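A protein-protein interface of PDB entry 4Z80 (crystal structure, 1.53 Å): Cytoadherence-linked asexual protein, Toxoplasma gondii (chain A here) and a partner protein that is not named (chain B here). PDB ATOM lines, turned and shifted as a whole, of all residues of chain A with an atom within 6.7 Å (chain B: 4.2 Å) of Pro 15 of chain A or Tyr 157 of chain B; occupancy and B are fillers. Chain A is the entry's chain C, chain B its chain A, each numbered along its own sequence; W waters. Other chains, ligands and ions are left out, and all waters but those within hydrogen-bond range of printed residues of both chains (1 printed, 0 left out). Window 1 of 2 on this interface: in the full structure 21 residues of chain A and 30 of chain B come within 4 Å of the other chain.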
ATOM      1  N   ASN A   9     -17.763  -5.723  11.635  1.00  0.00           N
ATOM      2  CA  ASN A   9     -18.274  -6.848  10.878  1.00  0.00           C
ATOM      3  C   ASN A   9     -19.792  -6.876  10.939  1.00  0.00           C
ATOM      4  O   ASN A   9     -20.414  -6.039  11.587  1.00  0.00           O
ATOM      5  CB  ASN A   9     -17.671  -8.180  11.355  1.00  0.00           C
ATOM      6  CG  ASN A   9     -18.063  -8.568  12.778  1.00  0.00           C
ATOM      7  OD1 ASN A   9     -18.872  -7.920  13.440  1.00  0.00           O
ATOM      8  ND2 ASN A   9     -17.463  -9.658  13.253  1.00  0.00           N
ATOM      9  N   GLN A  10     -20.383  -7.827  10.234  1.00  0.00           N
ATOM     10  CA  GLN A  10     -21.831  -7.841  10.086  1.00  0.00           C
ATOM     11  C   GLN A  10     -22.540  -8.161  11.395  1.00  0.00           C
ATOM     12  O   GLN A  10     -23.625  -7.643  11.649  1.00  0.00           O
ATOM     13  CB  GLN A  10     -22.245  -8.839   9.004  1.00  0.00           C
ATOM     14  CG  GLN A  10     -21.835  -8.401   7.611  1.00  0.00           C
ATOM     15  CD  GLN A  10     -22.553  -7.140   7.155  1.00  0.00           C
ATOM     16  OE1 GLN A  10     -23.714  -6.910   7.496  1.00  0.00           O
ATOM     17  NE2 GLN A  10     -21.855  -6.313   6.387  1.00  0.00           N
ATOM     18  N   SER A  11     -21.944  -8.995  12.241  1.00  0.00           N
ATOM     19  CA  SER A  11     -22.599  -9.329  13.500  1.00  0.00           C
ATOM     20  C   SER A  11     -22.598  -8.132  14.454  1.00  0.00           C
ATOM     21  O   SER A  11     -23.510  -7.982  15.271  1.00  0.00           O
ATOM     22  CB  SER A  11     -21.938 -10.545  14.144  1.00  0.00           C
ATOM     23  OG  SER A  11     -22.346 -11.723  13.469  1.00  0.00           O
ATOM     24  N   SER A  12     -21.592  -7.269  14.337  1.00  0.00           N
ATOM     25  CA  SER A  12     -21.547  -6.023  15.103  1.00  0.00           C
ATOM     26  C   SER A  12     -22.625  -5.056  14.632  1.00  0.00           C
ATOM     27  O   SER A  12     -23.301  -4.410  15.439  1.00  0.00           O
ATOM     28  CB  SER A  12     -20.163  -5.375  14.982  1.00  0.00           C
ATOM     29  OG  SER A  12     -20.170  -4.031  15.445  1.00  0.00           O
ATOM     30  N   LEU A  13     -22.787  -4.964  13.319  1.00  0.00           N
ATOM     31  CA  LEU A  13     -23.786  -4.079  12.739  1.00  0.00           C
ATOM     32  C   LEU A  13     -25.208  -4.594  12.989  1.00  0.00           C
ATOM     33  O   LEU A  13     -26.155  -3.808  13.055  1.00  0.00           O
ATOM     34  CB  LEU A  13     -23.534  -3.930  11.238  1.00  0.00           C
ATOM     35  CG  LEU A  13     -24.525  -3.073  10.453  1.00  0.00           C
ATOM     36  CD1 LEU A  13     -24.580  -1.664  11.018  1.00  0.00           C
ATOM     37  CD2 LEU A  13     -24.136  -3.058   8.979  1.00  0.00           C
ATOM     38  N   ALA A  14     -25.349  -5.908  13.144  1.00  0.00           N
ATOM     39  CA  ALA A  14     -26.669  -6.553  13.161  1.00  0.00           C
ATOM     40  C   ALA A  14     -27.687  -5.913  14.127  1.00  0.00           C
ATOM     41  O   ALA A  14     -28.816  -5.651  13.725  1.00  0.00           O
ATOM     42  CB  ALA A  14     -26.524  -8.043  13.474  1.00  0.00           C
ATOM     43  N   PRO A  15     -27.311  -5.665  15.394  1.00  0.00           N
ATOM     44  CA  PRO A  15     -28.317  -5.087  16.302  1.00  0.00           C
ATOM     45  C   PRO A  15     -28.856  -3.732  15.849  1.00  0.00           C
ATOM     46  O   PRO A  15     -29.960  -3.357  16.229  1.00  0.00           O
ATOM     47  CB  PRO A  15     -27.566  -4.952  17.639  1.00  0.00           C
ATOM     48  CG  PRO A  15     -26.135  -5.239  17.343  1.00  0.00           C
ATOM     49  CD  PRO A  15     -26.079  -6.046  16.102  1.00  0.00           C
ATOM     50  N   GLU A  16     -28.091  -3.016  15.038  1.00  0.00           N
ATOM     51  CA  GLU A  16     -28.485  -1.686  14.586  1.00  0.00           C
ATOM     52  C   GLU A  16     -29.425  -1.757  13.376  1.00  0.00           C
ATOM     53  O   GLU A  16     -30.034  -0.755  12.996  1.00  0.00           O
ATOM     54  CB  GLU A  16     -27.239  -0.865  14.250  1.00  0.00           C
ATOM     55  CG  GLU A  16     -26.121  -1.000  15.293  1.00  0.00           C
ATOM     56  CD  GLU A  16     -26.602  -0.683  16.697  1.00  0.00           C
ATOM     57  OE1 GLU A  16     -27.531   0.141  16.834  1.00  0.00           O
ATOM     58  OE2 GLU A  16     -26.058  -1.260  17.661  1.00  0.00           O
ATOM     59  N   LEU A  17     -29.531  -2.945  12.782  1.00  0.00           N
ATOM     60  CA  LEU A  17     -30.423  -3.180  11.645  1.00  0.00           C
ATOM     61  C   LEU A  17     -31.675  -3.939  12.060  1.00  0.00           C
ATOM     62  O   LEU A  17     -32.684  -3.909  11.362  1.00  0.00           O
ATOM     63  CB  LEU A  17     -29.705  -3.971  10.544  1.00  0.00           C
ATOM     64  CG  LEU A  17     -28.427  -3.365   9.969  1.00  0.00           C
ATOM     65  CD1 LEU A  17     -27.876  -4.249   8.856  1.00  0.00           C
ATOM     66  CD2 LEU A  17     -28.684  -1.958   9.465  1.00  0.00           C
ATOM     67  N   SER A  18     -31.593  -4.644  13.182  1.00  0.00           N
ATOM     68  CA  SER A  18     -32.660  -5.516  13.632  1.00  0.00           C
ATOM     69  C   SER A  18     -33.941  -4.755  13.920  1.00  0.00           C
ATOM     70  O   SER A  18     -33.908  -3.611  14.367  1.00  0.00           O
ATOM     71  CB  SER A  18     -32.226  -6.268  14.892  1.00  0.00           C
ATOM     72  OG  SER A  18     -33.269  -7.084  15.396  1.00  0.00           O
ATOM     73  N   GLY A  19     -35.069  -5.402  13.659  1.00  0.00           N
ATOM     74  CA  GLY A  19     -36.345  -4.850  14.062  1.00  0.00           C
ATOM     75  C   GLY A  19     -36.545  -4.955  15.565  1.00  0.00           C
ATOM     76  O   GLY A  19     -37.383  -4.254  16.128  1.00  0.00           O
ATOM     77  N   CYS A  20     -35.772  -5.827  16.214  1.00  0.00           N
ATOM     78  CA  CYS A  20     -35.916  -6.086  17.649  1.00  0.00           C
ATOM     79  C   CYS A  20     -34.583  -6.045  18.402  1.00  0.00           C
ATOM     80  O   CYS A  20     -34.157  -7.057  18.968  1.00  0.00           O
ATOM     81  CB  CYS A  20     -36.573  -7.450  17.870  1.00  0.00           C
ATOM     82  SG  CYS A  20     -38.280  -7.558  17.274  1.00  0.00           S
ATOM     83  N   PRO A  21     -33.928  -4.876  18.423  1.00  0.00           N
ATOM     84  CA  PRO A  21     -32.661  -4.748  19.150  1.00  0.00           C
ATOM     85  C   PRO A  21     -32.869  -4.850  20.658  1.00  0.00           C
ATOM     86  O   PRO A  21     -33.985  -4.632  21.122  1.00  0.00           O
ATOM     87  CB  PRO A  21     -32.172  -3.356  18.761  1.00  0.00           C
ATOM     88  CG  PRO A  21     -33.432  -2.591  18.464  1.00  0.00           C
ATOM     89  CD  PRO A  21     -34.363  -3.595  17.839  1.00  0.00           C
ATOM     90  N   PRO A  22     -31.800  -5.137  21.419  1.00  0.00           N
ATOM     91  CA  PRO A  22     -30.421  -5.297  20.946  1.00  0.00           C
ATOM     92  C   PRO A  22     -29.989  -6.734  20.630  1.00  0.00           C
ATOM     93  O   PRO A  22     -28.878  -6.901  20.117  1.00  0.00           O
ATOM     94  CB  PRO A  22     -29.606  -4.755  22.120  1.00  0.00           C
ATOM     95  CG  PRO A  22     -30.412  -5.121  23.314  1.00  0.00           C
ATOM     96  CD  PRO A  22     -31.856  -4.988  22.885  1.00  0.00           C
ATOM     97  N   MET A  23     -30.816  -7.733  20.936  1.00  0.00           N
ATOM     98  CA  MET A  23     -30.422  -9.126  20.733  1.00  0.00           C
ATOM     99  C   MET A  23     -31.281  -9.858  19.704  1.00  0.00           C
ATOM    100  O   MET A  23     -30.932 -10.962  19.286  1.00  0.00           O
ATOM    101  CB  MET A  23     -30.467  -9.878  22.061  1.00  0.00           C
ATOM    102  CG  MET A  23     -29.346  -9.496  23.015  1.00  0.00           C
ATOM    103  SD  MET A  23     -27.794 -10.347  22.650  1.00  0.00           S
ATOM    104  CE  MET A  23     -28.225 -12.021  23.139  1.00  0.00           C
ATOM    105  N   GLY A  24     -32.398  -9.252  19.307  1.00  0.00           N
ATOM    106  CA  GLY A  24     -33.278  -9.847  18.313  1.00  0.00           C
ATOM    107  C   GLY A  24     -34.606 -10.346  18.868  1.00  0.00           C
ATOM    108  O   GLY A  24     -35.370 -10.997  18.156  1.00  0.00           O
ATOM    109  N   MET B 126     -19.384  -7.449  26.207  1.00  0.00           N
ATOM    110  CA  MET B 126     -20.831  -7.595  26.408  1.00  0.00           C
ATOM    111  C   MET B 126     -21.339  -6.646  27.491  1.00  0.00           C
ATOM    112  O   MET B 126     -20.793  -6.613  28.588  1.00  0.00           O
ATOM    113  CB  MET B 126     -21.185  -9.038  26.794  1.00  0.00           C
ATOM    114  CG  MET B 126     -20.734 -10.098  25.791  1.00  0.00           C
ATOM    115  SD  MET B 126     -21.441  -9.837  24.148  1.00  0.00           S
ATOM    116  CE  MET B 126     -20.816 -11.284  23.283  1.00  0.00           C
ATOM    117  N   HIS B 128     -22.622  -5.605  23.634  1.00  0.00           N
ATOM    118  CA  HIS B 128     -22.008  -4.940  22.500  1.00  0.00           C
ATOM    119  C   HIS B 128     -22.848  -3.755  22.055  1.00  0.00           C
ATOM    120  O   HIS B 128     -22.320  -2.750  21.590  1.00  0.00           O
ATOM    121  CB  HIS B 128     -21.824  -5.930  21.352  1.00  0.00           C
ATOM    122  CG  HIS B 128     -21.151  -5.339  20.159  1.00  0.00           C
ATOM    123  ND1 HIS B 128     -19.825  -4.967  20.164  1.00  0.00           N
ATOM    124  CD2 HIS B 128     -21.628  -5.025  18.933  1.00  0.00           C
ATOM    125  CE1 HIS B 128     -19.510  -4.460  18.986  1.00  0.00           C
ATOM    126  NE2 HIS B 128     -20.586  -4.483  18.222  1.00  0.00           N
ATOM    127  N   SER B 129     -24.162  -3.892  22.204  1.00  0.00           N
ATOM    128  CA  SER B 129     -25.100  -2.822  21.878  1.00  0.00           C
ATOM    129  C   SER B 129     -26.211  -2.791  22.911  1.00  0.00           C
ATOM    130  O   SER B 129     -26.594  -3.827  23.455  1.00  0.00           O
ATOM    131  CB  SER B 129     -25.691  -3.013  20.478  1.00  0.00           C
ATOM    132  OG  SER B 129     -26.740  -2.084  20.237  1.00  0.00           O
ATOM    133  N   GLY B 156     -22.781 -17.158  23.641  1.00  0.00           N
ATOM    134  CA  GLY B 156     -23.441 -16.872  22.385  1.00  0.00           C
ATOM    135  C   GLY B 156     -23.607 -15.380  22.212  1.00  0.00           C
ATOM    136  O   GLY B 156     -23.223 -14.592  23.083  1.00  0.00           O
ATOM    137  N   TYR B 157     -24.174 -14.984  21.079  1.00  0.00           N
ATOM    138  CA  TYR B 157     -24.367 -13.574  20.762  1.00  0.00           C
ATOM    139  C   TYR B 157     -25.498 -13.467  19.737  1.00  0.00           C
ATOM    140  O   TYR B 157     -25.487 -14.171  18.727  1.00  0.00           O
ATOM    141  CB  TYR B 157     -23.070 -12.943  20.233  1.00  0.00           C
ATOM    142  CG  TYR B 157     -23.248 -11.527  19.748  1.00  0.00           C
ATOM    143  CD1 TYR B 157     -23.560 -10.499  20.630  1.00  0.00           C
ATOM    144  CD2 TYR B 157     -23.111 -11.217  18.404  1.00  0.00           C
ATOM    145  CE1 TYR B 157     -23.734  -9.202  20.175  1.00  0.00           C
ATOM    146  CE2 TYR B 157     -23.277  -9.928  17.947  1.00  0.00           C
ATOM    147  CZ  TYR B 157     -23.594  -8.930  18.827  1.00  0.00           C
ATOM    148  OH  TYR B 157     -23.765  -7.649  18.348  1.00  0.00           O
ATOM    149  N   LEU B 158     -26.476 -12.603  20.030  1.00  0.00           N
ATOM    150  CA  LEU B 158     -27.736 -12.490  19.276  1.00  0.00           C
ATOM    151  C   LEU B 158     -28.519 -13.798  19.387  1.00  0.00           C
ATOM    152  O   LEU B 158     -28.060 -14.751  20.007  1.00  0.00           O
ATOM    153  CB  LEU B 158     -27.482 -12.119  17.806  1.00  0.00           C
ATOM    154  CG  LEU B 158     -26.631 -10.863  17.609  1.00  0.00           C
ATOM    155  CD1 LEU B 158     -26.374 -10.594  16.134  1.00  0.00           C
ATOM    156  CD2 LEU B 158     -27.271  -9.655  18.271  1.00  0.00           C
ATOM    157  N   PHE B 194     -28.756 -19.712  19.726  1.00  0.00           N
ATOM    158  CA  PHE B 194     -28.423 -19.341  21.097  1.00  0.00           C
ATOM    159  C   PHE B 194     -29.720 -19.248  21.882  1.00  0.00           C
ATOM    160  O   PHE B 194     -29.930 -19.981  22.845  1.00  0.00           O
ATOM    161  CB  PHE B 194     -27.664 -18.009  21.126  1.00  0.00           C
ATOM    162  CG  PHE B 194     -27.236 -17.551  22.508  1.00  0.00           C
ATOM    163  CD1 PHE B 194     -27.011 -18.445  23.542  1.00  0.00           C
ATOM    164  CD2 PHE B 194     -27.046 -16.202  22.751  1.00  0.00           C
ATOM    165  CE1 PHE B 194     -26.605 -17.990  24.791  1.00  0.00           C
ATOM    166  CE2 PHE B 194     -26.639 -15.746  23.996  1.00  0.00           C
ATOM    167  CZ  PHE B 194     -26.423 -16.637  25.010  1.00  0.00           C
ATOM    168  N   PHE B 211     -23.656 -21.383  21.687  1.00  0.00           N
ATOM    169  CA  PHE B 211     -22.895 -21.708  20.480  1.00  0.00           C
ATOM    170  C   PHE B 211     -21.845 -22.802  20.727  1.00  0.00           C
ATOM    171  O   PHE B 211     -21.342 -23.397  19.775  1.00  0.00           O
ATOM    172  CB  PHE B 211     -22.191 -20.473  19.915  1.00  0.00           C
ATOM    173  CG  PHE B 211     -23.117 -19.425  19.338  1.00  0.00           C
ATOM    174  CD1 PHE B 211     -24.461 -19.684  19.084  1.00  0.00           C
ATOM    175  CD2 PHE B 211     -22.626 -18.166  19.038  1.00  0.00           C
ATOM    176  CE1 PHE B 211     -25.278 -18.700  18.541  1.00  0.00           C
ATOM    177  CE2 PHE B 211     -23.441 -17.185  18.505  1.00  0.00           C
ATOM    178  CZ  PHE B 211     -24.765 -17.452  18.257  1.00  0.00           C
ATOM    179  N   TYR B 220     -21.579 -14.605  31.064  1.00  0.00           N
ATOM    180  CA  TYR B 220     -22.140 -13.268  31.053  1.00  0.00           C
ATOM    181  C   TYR B 220     -23.657 -13.326  31.068  1.00  0.00           C
ATOM    182  O   TYR B 220     -24.258 -14.307  30.639  1.00  0.00           O
ATOM    183  CB  TYR B 220     -21.626 -12.468  29.849  1.00  0.00           C
ATOM    184  CG  TYR B 220     -22.359 -12.595  28.520  1.00  0.00           C
ATOM    185  CD1 TYR B 220     -22.178 -13.697  27.691  1.00  0.00           C
ATOM    186  CD2 TYR B 220     -23.165 -11.559  28.062  1.00  0.00           C
ATOM    187  CE1 TYR B 220     -22.813 -13.778  26.463  1.00  0.00           C
ATOM    188  CE2 TYR B 220     -23.800 -11.632  26.838  1.00  0.00           C
ATOM    189  CZ  TYR B 220     -23.626 -12.744  26.046  1.00  0.00           C
ATOM    190  OH  TYR B 220     -24.256 -12.804  24.822  1.00  0.00           O
ATOM    191  N   CYS B 265     -19.773 -15.203  14.010  1.00  0.00           N
ATOM    192  CA  CYS B 265     -20.868 -15.097  14.969  1.00  0.00           C
ATOM    193  C   CYS B 265     -20.591 -14.054  16.043  1.00  0.00           C
ATOM    194  O   CYS B 265     -21.506 -13.631  16.740  1.00  0.00           O
ATOM    195  CB  CYS B 265     -21.121 -16.444  15.641  1.00  0.00           C
ATOM    196  SG  CYS B 265     -21.445 -17.816  14.508  1.00  0.00           S
ATOM    197  N   TRP B 266     -19.326 -13.660  16.189  1.00  0.00           N
ATOM    198  CA  TRP B 266     -18.935 -12.719  17.231  1.00  0.00           C
ATOM    199  C   TRP B 266     -18.804 -11.321  16.663  1.00  0.00           C
ATOM    200  O   TRP B 266     -18.383 -11.146  15.518  1.00  0.00           O
ATOM    201  CB  TRP B 266     -17.615 -13.138  17.882  1.00  0.00           C
ATOM    202  CG  TRP B 266     -17.590 -14.570  18.252  1.00  0.00           C
ATOM    203  CD1 TRP B 266     -16.775 -15.527  17.733  1.00  0.00           C
ATOM    204  CD2 TRP B 266     -18.423 -15.229  19.215  1.00  0.00           C
ATOM    205  NE1 TRP B 266     -17.040 -16.740  18.313  1.00  0.00           N
ATOM    206  CE2 TRP B 266     -18.048 -16.586  19.227  1.00  0.00           C
ATOM    207  CE3 TRP B 266     -19.445 -14.805  20.071  1.00  0.00           C
ATOM    208  CZ2 TRP B 266     -18.658 -17.525  20.063  1.00  0.00           C
ATOM    209  CZ3 TRP B 266     -20.050 -15.741  20.902  1.00  0.00           C
ATOM    210  CH2 TRP B 266     -19.655 -17.081  20.892  1.00  0.00           C
ATOM    211  N   PRO B 267     -19.148 -10.306  17.463  1.00  0.00           N
ATOM    212  CA  PRO B 267     -19.073  -8.939  16.953  1.00  0.00           C
ATOM    213  C   PRO B 267     -17.648  -8.404  16.939  1.00  0.00           C
ATOM    214  O   PRO B 267     -16.875  -8.685  17.862  1.00  0.00           O
ATOM    215  CB  PRO B 267     -19.929  -8.158  17.943  1.00  0.00           C
ATOM    216  CG  PRO B 267     -19.743  -8.879  19.220  1.00  0.00           C
ATOM    217  CD  PRO B 267     -19.607 -10.340  18.864  1.00  0.00           C
HETATM  218  O   HOH W   1     -25.185 -10.167  23.765  1.00  0.00           O
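Pro 15 of chain A touches two residues of chain B. Of chain A, only Ser 11 (3.1 Å) and Pro 15 (3.5 Å) come within 4 Å of Tyr 157 of chain B. Printed residues of chain B within 4 Å of Pro 22 of chain A: Ser 129 and Leu 158. Of the printed residues of chain B, Asn 9 of chain A touches Trp 266 and Pro 267. The nearest printed residue of chain B that does not touch Pro 15 of chain A is Leu 158 of chain B (4.4 Å). The nearest printed residue of chain B that does not touch Ala 14 of chain A is Tyr 157 of chain B (5.6 Å).
Pro 267 of chain B touches Asn 9 of chain A (CA to OD1, 3.7 Å). CD1 of Leu 158 of chain B touches O of Ser 11 of chain A, 3.97 Å away. Ser 11 of chain A touches Cys 265 of chain B. CB of Ser 11 of chain A touches O of Trp 266 of chain B, 3.9 Å away. CB of Pro 267 of chain B touches CA of Ser 12 of chain A, at 3.9 Å. Leu 158 of chain B touches Ala 14 of chain A. Pro 15 of chain A touches Ser 129 of chain B. CG of Pro 15 of chain A touches OH of Tyr 157 of chain B, at 3.5 Å. Pro 22 of chain A touches Ser 129 of chain B (CB to O, 3.4 Å). CD2 of Leu 158 of chain B touches O of Pro 22 of chain A (3.7 Å).
OG of Ser 12 of chain A is in hydrogen-bond range of NE2 of His 128 of chain B. OG of Ser 129 of chain B lies within hydrogen-bond range of OE2 of Glu 16 of chain A, 2.8 Å away. The backbone carbonyl oxygen (O) of Ser 11 of chain A sits at hydrogen-bond distance from the side-chain hydroxyl (OH) of Tyr 157 of chain B (3.1 Å). The backbone NH of Leu 158 of chain B lies close to the side-chain sulfur of Met 23 of chain A (3.7 Å). ND2 of Asn 9 of chain A lies within hydrogen-bond range of O of Trp 266 of chain B, at 2.9 Å.
Among the printed residues, 15 pairs touch across the chains.
The side-chain amide oxygen (OD1) of Asn 9 of chain A lies close to the backbone NH (N) of Ser 11 of chain A (3.5 Å). N of Ser 12 of chain A is in hydrogen-bond range of OD1 of Asn 9 of chain A (2.9 Å).
Water W1 lies within hydrogen-bond range of the side-chain sulfur (SD) of Met 23 of chain A (2.8 Å), the side-chain hydroxyl (OH) of Tyr 220 of chain B (3.0 Å) and the side-chain sulfur (SD) of Met 126 of chain B (3.8 Å).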
